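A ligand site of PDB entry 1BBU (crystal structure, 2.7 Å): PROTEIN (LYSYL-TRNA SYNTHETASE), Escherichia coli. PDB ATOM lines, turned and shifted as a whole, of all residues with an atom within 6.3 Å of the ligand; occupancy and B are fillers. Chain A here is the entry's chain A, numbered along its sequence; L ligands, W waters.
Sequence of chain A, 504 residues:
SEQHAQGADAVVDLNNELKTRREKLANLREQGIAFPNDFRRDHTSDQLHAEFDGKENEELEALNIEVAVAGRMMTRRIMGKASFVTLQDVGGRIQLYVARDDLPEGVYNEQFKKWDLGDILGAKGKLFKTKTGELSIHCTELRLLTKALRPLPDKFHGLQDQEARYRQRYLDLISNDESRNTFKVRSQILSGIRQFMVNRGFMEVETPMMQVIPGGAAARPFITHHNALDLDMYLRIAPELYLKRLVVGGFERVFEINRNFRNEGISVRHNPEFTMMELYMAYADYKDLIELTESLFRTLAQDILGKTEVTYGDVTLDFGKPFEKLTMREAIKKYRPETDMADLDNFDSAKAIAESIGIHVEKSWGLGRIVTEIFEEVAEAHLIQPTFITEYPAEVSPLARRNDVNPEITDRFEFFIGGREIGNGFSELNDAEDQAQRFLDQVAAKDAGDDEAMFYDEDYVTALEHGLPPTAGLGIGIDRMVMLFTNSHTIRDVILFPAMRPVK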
ATOM      1  N   GLY A 216     -35.076  14.443  19.041  1.00  0.00           N
ATOM      2  CA  GLY A 216     -34.195  15.087  18.078  1.00  0.00           C
ATOM      3  C   GLY A 216     -33.108  14.154  17.564  1.00  0.00           C
ATOM      4  O   GLY A 216     -32.191  14.587  16.875  1.00  0.00           O
ATOM      5  N   ALA A 217     -33.261  12.866  17.898  1.00  0.00           N
ATOM      6  CA  ALA A 217     -32.336  11.786  17.538  1.00  0.00           C
ATOM      7  C   ALA A 217     -32.926  10.466  18.068  1.00  0.00           C
ATOM      8  O   ALA A 217     -33.931  10.484  18.796  1.00  0.00           O
ATOM      9  CB  ALA A 217     -30.964  12.017  18.176  1.00  0.00           C
ATOM     10  N   ALA A 218     -32.311   9.349  17.703  1.00  0.00           N
ATOM     11  CA  ALA A 218     -32.754   8.035  18.174  1.00  0.00           C
ATOM     12  C   ALA A 218     -31.724   7.465  19.158  1.00  0.00           C
ATOM     13  O   ALA A 218     -30.607   7.141  18.753  1.00  0.00           O
ATOM     14  CB  ALA A 218     -32.947   7.099  17.000  1.00  0.00           C
ATOM     15  N   ILE A 237     -30.879  14.188  24.404  1.00  0.00           N
ATOM     16  CA  ILE A 237     -30.207  13.336  23.425  1.00  0.00           C
ATOM     17  C   ILE A 237     -29.832  14.200  22.220  1.00  0.00           C
ATOM     18  O   ILE A 237     -28.885  13.891  21.492  1.00  0.00           O
ATOM     19  CB  ILE A 237     -31.037  12.112  23.028  1.00  0.00           C
ATOM     20  CG1 ILE A 237     -32.259  12.511  22.223  1.00  0.00           C
ATOM     21  CG2 ILE A 237     -31.519  11.394  24.255  1.00  0.00           C
ATOM     22  CD1 ILE A 237     -33.100  11.309  21.809  1.00  0.00           C
ATOM     23  N   ALA A 238     -30.536  15.314  22.050  1.00  0.00           N
ATOM     24  CA  ALA A 238     -30.284  16.315  21.001  1.00  0.00           C
ATOM     25  C   ALA A 238     -31.112  17.548  21.323  1.00  0.00           C
ATOM     26  O   ALA A 238     -32.107  17.459  22.052  1.00  0.00           O
ATOM     27  CB  ALA A 238     -30.672  15.791  19.608  1.00  0.00           C
ATOM     28  N   PRO A 239     -30.704  18.714  20.838  1.00  0.00           N
ATOM     29  CA  PRO A 239     -31.419  19.978  21.039  1.00  0.00           C
ATOM     30  C   PRO A 239     -32.311  20.360  19.820  1.00  0.00           C
ATOM     31  O   PRO A 239     -32.939  21.420  19.815  1.00  0.00           O
ATOM     32  CB  PRO A 239     -30.272  20.966  21.193  1.00  0.00           C
ATOM     33  CG  PRO A 239     -29.328  20.498  20.138  1.00  0.00           C
ATOM     34  CD  PRO A 239     -29.335  18.972  20.345  1.00  0.00           C
ATOM     35  N   GLU A 240     -32.373  19.484  18.809  1.00  0.00           N
ATOM     36  CA  GLU A 240     -33.082  19.770  17.558  1.00  0.00           C
ATOM     37  C   GLU A 240     -34.427  20.513  17.649  1.00  0.00           C
ATOM     38  O   GLU A 240     -34.589  21.590  17.075  1.00  0.00           O
ATOM     39  CB  GLU A 240     -33.244  18.497  16.731  1.00  0.00           C
ATOM     40  CG  GLU A 240     -34.120  18.668  15.495  1.00  0.00           C
ATOM     41  CD  GLU A 240     -33.683  17.784  14.344  1.00  0.00           C
ATOM     42  OE1 GLU A 240     -32.480  17.675  14.112  1.00  0.00           O
ATOM     43  OE2 GLU A 240     -34.556  17.221  13.646  1.00  0.00           O
ATOM     44  N   LYS A 244     -35.433  24.439  16.445  1.00  0.00           N
ATOM     45  CA  LYS A 244     -36.411  24.687  15.397  1.00  0.00           C
ATOM     46  C   LYS A 244     -37.461  25.679  15.888  1.00  0.00           C
ATOM     47  O   LYS A 244     -37.922  26.520  15.120  1.00  0.00           O
ATOM     48  CB  LYS A 244     -37.036  23.380  14.893  1.00  0.00           C
ATOM     49  CG  LYS A 244     -36.497  23.011  13.505  1.00  0.00           C
ATOM     50  CD  LYS A 244     -37.025  21.692  12.981  1.00  0.00           C
ATOM     51  CE  LYS A 244     -36.123  20.523  13.343  1.00  0.00           C
ATOM     52  NZ  LYS A 244     -36.658  19.225  12.822  1.00  0.00           N
ATOM     53  N   ASN A 260     -24.629  16.034  24.250  1.00  0.00           N
ATOM     54  CA  ASN A 260     -25.825  15.230  24.088  1.00  0.00           C
ATOM     55  C   ASN A 260     -25.476  14.081  24.988  1.00  0.00           C
ATOM     56  O   ASN A 260     -24.298  13.814  25.240  1.00  0.00           O
ATOM     57  CB  ASN A 260     -26.000  14.761  22.648  1.00  0.00           C
ATOM     58  CG  ASN A 260     -26.491  15.861  21.720  1.00  0.00           C
ATOM     59  OD1 ASN A 260     -27.247  16.756  22.116  1.00  0.00           O
ATOM     60  ND2 ASN A 260     -26.098  15.772  20.463  1.00  0.00           N
ATOM     61  N   ARG A 262     -26.412  10.081  25.677  1.00  0.00           N
ATOM     62  CA  ARG A 262     -27.092   8.899  25.203  1.00  0.00           C
ATOM     63  C   ARG A 262     -26.681   7.763  26.123  1.00  0.00           C
ATOM     64  O   ARG A 262     -25.498   7.496  26.292  1.00  0.00           O
ATOM     65  CB  ARG A 262     -26.731   8.663  23.726  1.00  0.00           C
ATOM     66  CG  ARG A 262     -27.109   9.868  22.835  1.00  0.00           C
ATOM     67  CD  ARG A 262     -26.909   9.713  21.314  1.00  0.00           C
ATOM     68  NE  ARG A 262     -27.096  11.009  20.638  1.00  0.00           N
ATOM     69  CZ  ARG A 262     -27.046  11.200  19.314  1.00  0.00           C
ATOM     70  NH1 ARG A 262     -26.844  10.177  18.496  1.00  0.00           N
ATOM     71  NH2 ARG A 262     -27.140  12.428  18.809  1.00  0.00           N
ATOM     72  N   MET A 276     -21.708  17.752  19.874  1.00  0.00           N
ATOM     73  CA  MET A 276     -22.357  17.879  18.579  1.00  0.00           C
ATOM     74  C   MET A 276     -22.637  19.343  18.219  1.00  0.00           C
ATOM     75  O   MET A 276     -22.838  20.191  19.096  1.00  0.00           O
ATOM     76  CB  MET A 276     -23.677  17.103  18.596  1.00  0.00           C
ATOM     77  CG  MET A 276     -24.313  16.888  17.224  1.00  0.00           C
ATOM     78  SD  MET A 276     -23.801  15.339  16.460  1.00  0.00           S
ATOM     79  CE  MET A 276     -24.834  14.138  17.360  1.00  0.00           C
ATOM     80  N   MET A 277     -22.568  19.658  16.932  1.00  0.00           N
ATOM     81  CA  MET A 277     -22.969  20.975  16.452  1.00  0.00           C
ATOM     82  C   MET A 277     -24.235  20.829  15.626  1.00  0.00           C
ATOM     83  O   MET A 277     -24.305  19.963  14.759  1.00  0.00           O
ATOM     84  CB  MET A 277     -21.899  21.614  15.575  1.00  0.00           C
ATOM     85  CG  MET A 277     -22.492  22.727  14.750  1.00  0.00           C
ATOM     86  SD  MET A 277     -21.356  23.722  13.763  1.00  0.00           S
ATOM     87  CE  MET A 277     -21.653  22.951  12.182  1.00  0.00           C
ATOM     88  N   GLU A 278     -25.251  21.629  15.933  1.00  0.00           N
ATOM     89  CA  GLU A 278     -26.422  21.707  15.063  1.00  0.00           C
ATOM     90  C   GLU A 278     -26.500  23.122  14.517  1.00  0.00           C
ATOM     91  O   GLU A 278     -26.089  24.083  15.181  1.00  0.00           O
ATOM     92  CB  GLU A 278     -27.711  21.346  15.809  1.00  0.00           C
ATOM     93  CG  GLU A 278     -27.768  19.894  16.256  1.00  0.00           C
ATOM     94  CD  GLU A 278     -29.186  19.401  16.466  1.00  0.00           C
ATOM     95  OE1 GLU A 278     -30.116  20.019  15.895  1.00  0.00           O
ATOM     96  OE2 GLU A 278     -29.383  18.377  17.165  1.00  0.00           O
ATOM     97  N   LEU A 279     -26.916  23.240  13.269  1.00  0.00           N
ATOM     98  CA  LEU A 279     -27.065  24.552  12.678  1.00  0.00           C
ATOM     99  C   LEU A 279     -28.289  24.469  11.777  1.00  0.00           C
ATOM    100  O   LEU A 279     -28.540  23.429  11.148  1.00  0.00           O
ATOM    101  CB  LEU A 279     -25.829  24.945  11.884  1.00  0.00           C
ATOM    102  CG  LEU A 279     -25.612  24.199  10.582  1.00  0.00           C
ATOM    103  CD1 LEU A 279     -26.253  24.960   9.435  1.00  0.00           C
ATOM    104  CD2 LEU A 279     -24.136  24.064  10.336  1.00  0.00           C
ATOM    105  N   TYR A 280     -29.071  25.536  11.762  1.00  0.00           N
ATOM    106  CA  TYR A 280     -30.284  25.607  10.972  1.00  0.00           C
ATOM    107  C   TYR A 280     -30.300  26.879  10.168  1.00  0.00           C
ATOM    108  O   TYR A 280     -29.843  27.925  10.635  1.00  0.00           O
ATOM    109  CB  TYR A 280     -31.496  25.539  11.887  1.00  0.00           C
ATOM    110  CG  TYR A 280     -31.668  24.193  12.528  1.00  0.00           C
ATOM    111  CD1 TYR A 280     -30.921  23.825  13.632  1.00  0.00           C
ATOM    112  CD2 TYR A 280     -32.533  23.250  11.974  1.00  0.00           C
ATOM    113  CE1 TYR A 280     -31.021  22.551  14.172  1.00  0.00           C
ATOM    114  CE2 TYR A 280     -32.633  21.975  12.514  1.00  0.00           C
ATOM    115  CZ  TYR A 280     -31.874  21.623  13.607  1.00  0.00           C
ATOM    116  OH  TYR A 280     -31.933  20.345  14.097  1.00  0.00           O
ATOM    117  N   LEU A 399     -38.131  13.338  11.088  1.00  0.00           N
ATOM    118  CA  LEU A 399     -38.161  14.792  11.169  1.00  0.00           C
ATOM    119  C   LEU A 399     -37.763  15.440   9.831  1.00  0.00           C
ATOM    120  O   LEU A 399     -37.404  16.631   9.766  1.00  0.00           O
ATOM    121  CB  LEU A 399     -37.187  15.277  12.271  1.00  0.00           C
ATOM    122  CG  LEU A 399     -37.400  14.697  13.680  1.00  0.00           C
ATOM    123  CD1 LEU A 399     -36.188  14.953  14.535  1.00  0.00           C
ATOM    124  CD2 LEU A 399     -38.628  15.280  14.319  1.00  0.00           C
ATOM    125  N   GLU A 421     -19.655   7.829  10.306  1.00  0.00           N
ATOM    126  CA  GLU A 421     -20.621   8.924  10.084  1.00  0.00           C
ATOM    127  C   GLU A 421     -20.177  10.193  10.804  1.00  0.00           C
ATOM    128  O   GLU A 421     -20.143  10.245  12.027  1.00  0.00           O
ATOM    129  CB  GLU A 421     -22.015   8.552  10.584  1.00  0.00           C
ATOM    130  CG  GLU A 421     -23.053   9.601  10.208  1.00  0.00           C
ATOM    131  CD  GLU A 421     -24.329   9.498  11.011  1.00  0.00           C
ATOM    132  OE1 GLU A 421     -24.965   8.410  10.995  1.00  0.00           O
ATOM    133  OE2 GLU A 421     -24.710  10.505  11.649  1.00  0.00           O
ATOM    134  N   ASN A 424     -24.961  14.604   9.411  1.00  0.00           N
ATOM    135  CA  ASN A 424     -26.368  14.252   9.251  1.00  0.00           C
ATOM    136  C   ASN A 424     -27.147  15.537   8.975  1.00  0.00           C
ATOM    137  O   ASN A 424     -27.017  16.511   9.715  1.00  0.00           O
ATOM    138  CB  ASN A 424     -26.890  13.621  10.543  1.00  0.00           C
ATOM    139  CG  ASN A 424     -28.379  13.304  10.483  1.00  0.00           C
ATOM    140  OD1 ASN A 424     -28.962  13.197   9.394  1.00  0.00           O
ATOM    141  ND2 ASN A 424     -28.999  13.143  11.655  1.00  0.00           N
ATOM    142  N   GLY A 425     -27.980  15.537   7.943  1.00  0.00           N
ATOM    143  CA  GLY A 425     -28.752  16.726   7.618  1.00  0.00           C
ATOM    144  C   GLY A 425     -29.955  16.471   6.731  1.00  0.00           C
ATOM    145  O   GLY A 425     -29.961  15.538   5.928  1.00  0.00           O
ATOM    146  N   PHE A 426     -30.992  17.299   6.860  1.00  0.00           N
ATOM    147  CA  PHE A 426     -32.167  17.214   5.990  1.00  0.00           C
ATOM    148  C   PHE A 426     -32.968  18.490   5.820  1.00  0.00           C
ATOM    149  O   PHE A 426     -32.755  19.480   6.545  1.00  0.00           O
ATOM    150  CB  PHE A 426     -33.096  16.069   6.425  1.00  0.00           C
ATOM    151  CG  PHE A 426     -33.284  15.945   7.902  1.00  0.00           C
ATOM    152  CD1 PHE A 426     -33.897  16.936   8.635  1.00  0.00           C
ATOM    153  CD2 PHE A 426     -32.843  14.806   8.571  1.00  0.00           C
ATOM    154  CE1 PHE A 426     -34.083  16.798  10.010  1.00  0.00           C
ATOM    155  CE2 PHE A 426     -33.021  14.661   9.944  1.00  0.00           C
ATOM    156  CZ  PHE A 426     -33.638  15.654  10.657  1.00  0.00           C
ATOM    157  N   GLU A 428     -36.009  20.200   6.597  1.00  0.00           N
ATOM    158  CA  GLU A 428     -36.864  20.028   7.783  1.00  0.00           C
ATOM    159  C   GLU A 428     -38.354  19.812   7.506  1.00  0.00           C
ATOM    160  O   GLU A 428     -38.942  20.488   6.659  1.00  0.00           O
ATOM    161  CB  GLU A 428     -36.711  21.261   8.670  1.00  0.00           C
ATOM    162  CG  GLU A 428     -35.278  21.552   8.994  1.00  0.00           C
ATOM    163  CD  GLU A 428     -34.601  20.403   9.729  1.00  0.00           C
ATOM    164  OE1 GLU A 428     -35.324  19.599  10.373  1.00  0.00           O
ATOM    165  OE2 GLU A 428     -33.367  20.310   9.655  1.00  0.00           O
ATOM    166  N   ALA A 472     -33.446  24.040   6.479  1.00  0.00           N
ATOM    167  CA  ALA A 472     -32.536  22.905   6.373  1.00  0.00           C
ATOM    168  C   ALA A 472     -31.660  22.889   7.621  1.00  0.00           C
ATOM    169  O   ALA A 472     -31.108  23.920   8.017  1.00  0.00           O
ATOM    170  CB  ALA A 472     -31.674  23.037   5.142  1.00  0.00           C
ATOM    171  N   GLY A 473     -31.557  21.723   8.251  1.00  0.00           N
ATOM    172  CA  GLY A 473     -30.734  21.598   9.440  1.00  0.00           C
ATOM    173  C   GLY A 473     -29.601  20.604   9.270  1.00  0.00           C
ATOM    174  O   GLY A 473     -29.771  19.581   8.616  1.00  0.00           O
ATOM    175  N   LEU A 474     -28.471  20.875   9.927  1.00  0.00           N
ATOM    176  CA  LEU A 474     -27.273  20.066   9.850  1.00  0.00           C
ATOM    177  C   LEU A 474     -26.698  19.741  11.226  1.00  0.00           C
ATOM    178  O   LEU A 474     -26.467  20.640  12.033  1.00  0.00           O
ATOM    179  CB  LEU A 474     -26.216  20.840   9.067  1.00  0.00           C
ATOM    180  CG  LEU A 474     -24.866  20.152   8.897  1.00  0.00           C
ATOM    181  CD1 LEU A 474     -25.065  18.853   8.137  1.00  0.00           C
ATOM    182  CD2 LEU A 474     -23.937  21.065   8.139  1.00  0.00           C
ATOM    183  N   GLY A 475     -26.437  18.463  11.470  1.00  0.00           N
ATOM    184  CA  GLY A 475     -25.761  18.023  12.685  1.00  0.00           C
ATOM    185  C   GLY A 475     -24.390  17.462  12.337  1.00  0.00           C
ATOM    186  O   GLY A 475     -24.214  16.787  11.314  1.00  0.00           O
ATOM    187  N   ILE A 476     -23.406  17.702  13.204  1.00  0.00           N
ATOM    188  CA  ILE A 476     -22.025  17.268  12.965  1.00  0.00           C
ATOM    189  C   ILE A 476     -21.335  16.795  14.247  1.00  0.00           C
ATOM    190  O   ILE A 476     -21.289  17.530  15.231  1.00  0.00           O
ATOM    191  CB  ILE A 476     -21.208  18.417  12.358  1.00  0.00           C
ATOM    192  CG1 ILE A 476     -21.546  18.573  10.883  1.00  0.00           C
ATOM    193  CG2 ILE A 476     -19.705  18.226  12.583  1.00  0.00           C
ATOM    194  CD1 ILE A 476     -20.807  19.710  10.250  1.00  0.00           C
HETATM  195  N1  LIG L   1     -30.362  16.218  15.596  1.00  0.00           N
HETATM  196  C1  LIG L   1     -29.546  15.531  14.600  1.00  0.00           C
HETATM  197  C2  LIG L   1     -28.681  14.408  15.188  1.00  0.00           C
HETATM  198  O1  LIG L   1     -28.661  14.253  16.429  1.00  0.00           O
HETATM  199  C3  LIG L   1     -28.667  16.549  13.849  1.00  0.00           C
HETATM  200  C4  LIG L   1     -29.433  17.559  12.979  1.00  0.00           C
HETATM  201  C5  LIG L   1     -30.264  16.868  11.886  1.00  0.00           C
HETATM  202  C6  LIG L   1     -30.893  17.891  10.938  1.00  0.00           C
HETATM  203  N2  LIG L   1     -32.080  18.551  11.504  1.00  0.00           N
HETATM  204  O2  LIG L   1     -28.032  13.669  14.405  1.00  0.00           O
HETATM  205  O   HOH W   1     -27.319  16.531  17.957  1.00  0.00           O
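OH of Tyr 280 lies within hydrogen-bond range of OE1 of Glu 240 (2.7 Å). The side-chain carboxylate of Glu 240 lies within salt-bridge range of the side-chain amino group of Lys 244 (3.0 Å). The side-chain carboxylate (OE1) of Glu 278 sits at hydrogen-bond distance from the side-chain hydroxyl (OH) of Tyr 280 (2.6 Å). N of Gly 473 sits at hydrogen-bond distance from OE2 of Glu 428 (2.7 Å). The side-chain carboxylate of Glu 428 is in salt-bridge range of the side-chain amino group of Lys 244, 2.8 Å away. N of Gly 473 lies within hydrogen-bond range of O of Phe 426 (3.1 Å). The guanidinium group (NE) of Arg 262 is in hydrogen-bond range of the backbone carbonyl oxygen (O) of Ile 237 (3.5 Å). The backbone carbonyl oxygen (O) of Leu 279 sits at hydrogen-bond distance from the backbone NH (N) of Leu 474, at 2.8 Å.
O of Gly 216 is in hydrogen-bond range of N1 of the ligand, 2.8 Å away. OE1 of Glu 240 is in salt-bridge range of N2 of the ligand (2.8 Å). OE2 of Glu 278 is in salt-bridge range of N1 of the ligand (2.8 Å). N2 of the ligand lies within salt-bridge range of OE2 of Glu 428. ND2 of Asn 424 is in hydrogen-bond range of O2 of the ligand. A nitrogen (N2) of the ligand lies within hydrogen-bond range of the side-chain hydroxyl (OH) of Tyr 280 (3.2 Å). The guanidinium group (NH2) of Arg 262 is in salt-bridge range of an oxygen (O1) of the ligand (3.4 Å).
Water W1 lies within hydrogen-bond range of the side-chain carboxylate of Glu 278 (2.9 Å), the side-chain amide nitrogen of Asn 260 (2.9 Å) and an oxygen (O1) of the ligand (3.1 Å).
Residues that only touch the ligand: Phe 426 (3.1 Å), Gly 473 (3.1 Å), Gly 475 (3.5 Å), Ala 217 (3.7 Å), Leu 474 (3.9 Å) and Met 276 (3.9 Å). Hydrophobic or aromatic side chains within 4 Å of the ligand: Ala 217, Met 276, Tyr 280 and Phe 426. 13 residues have an atom within 4 Å of the ligand: Gly 216, Ala 217, Glu 240, Arg 262, Met 276, Glu 278, Tyr 280, Asn 424, Phe 426, Glu 428, Gly 473, Leu 474 and Gly 475. Along chain A the residues within 4 Å of the ligand span positions 216 to 475.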
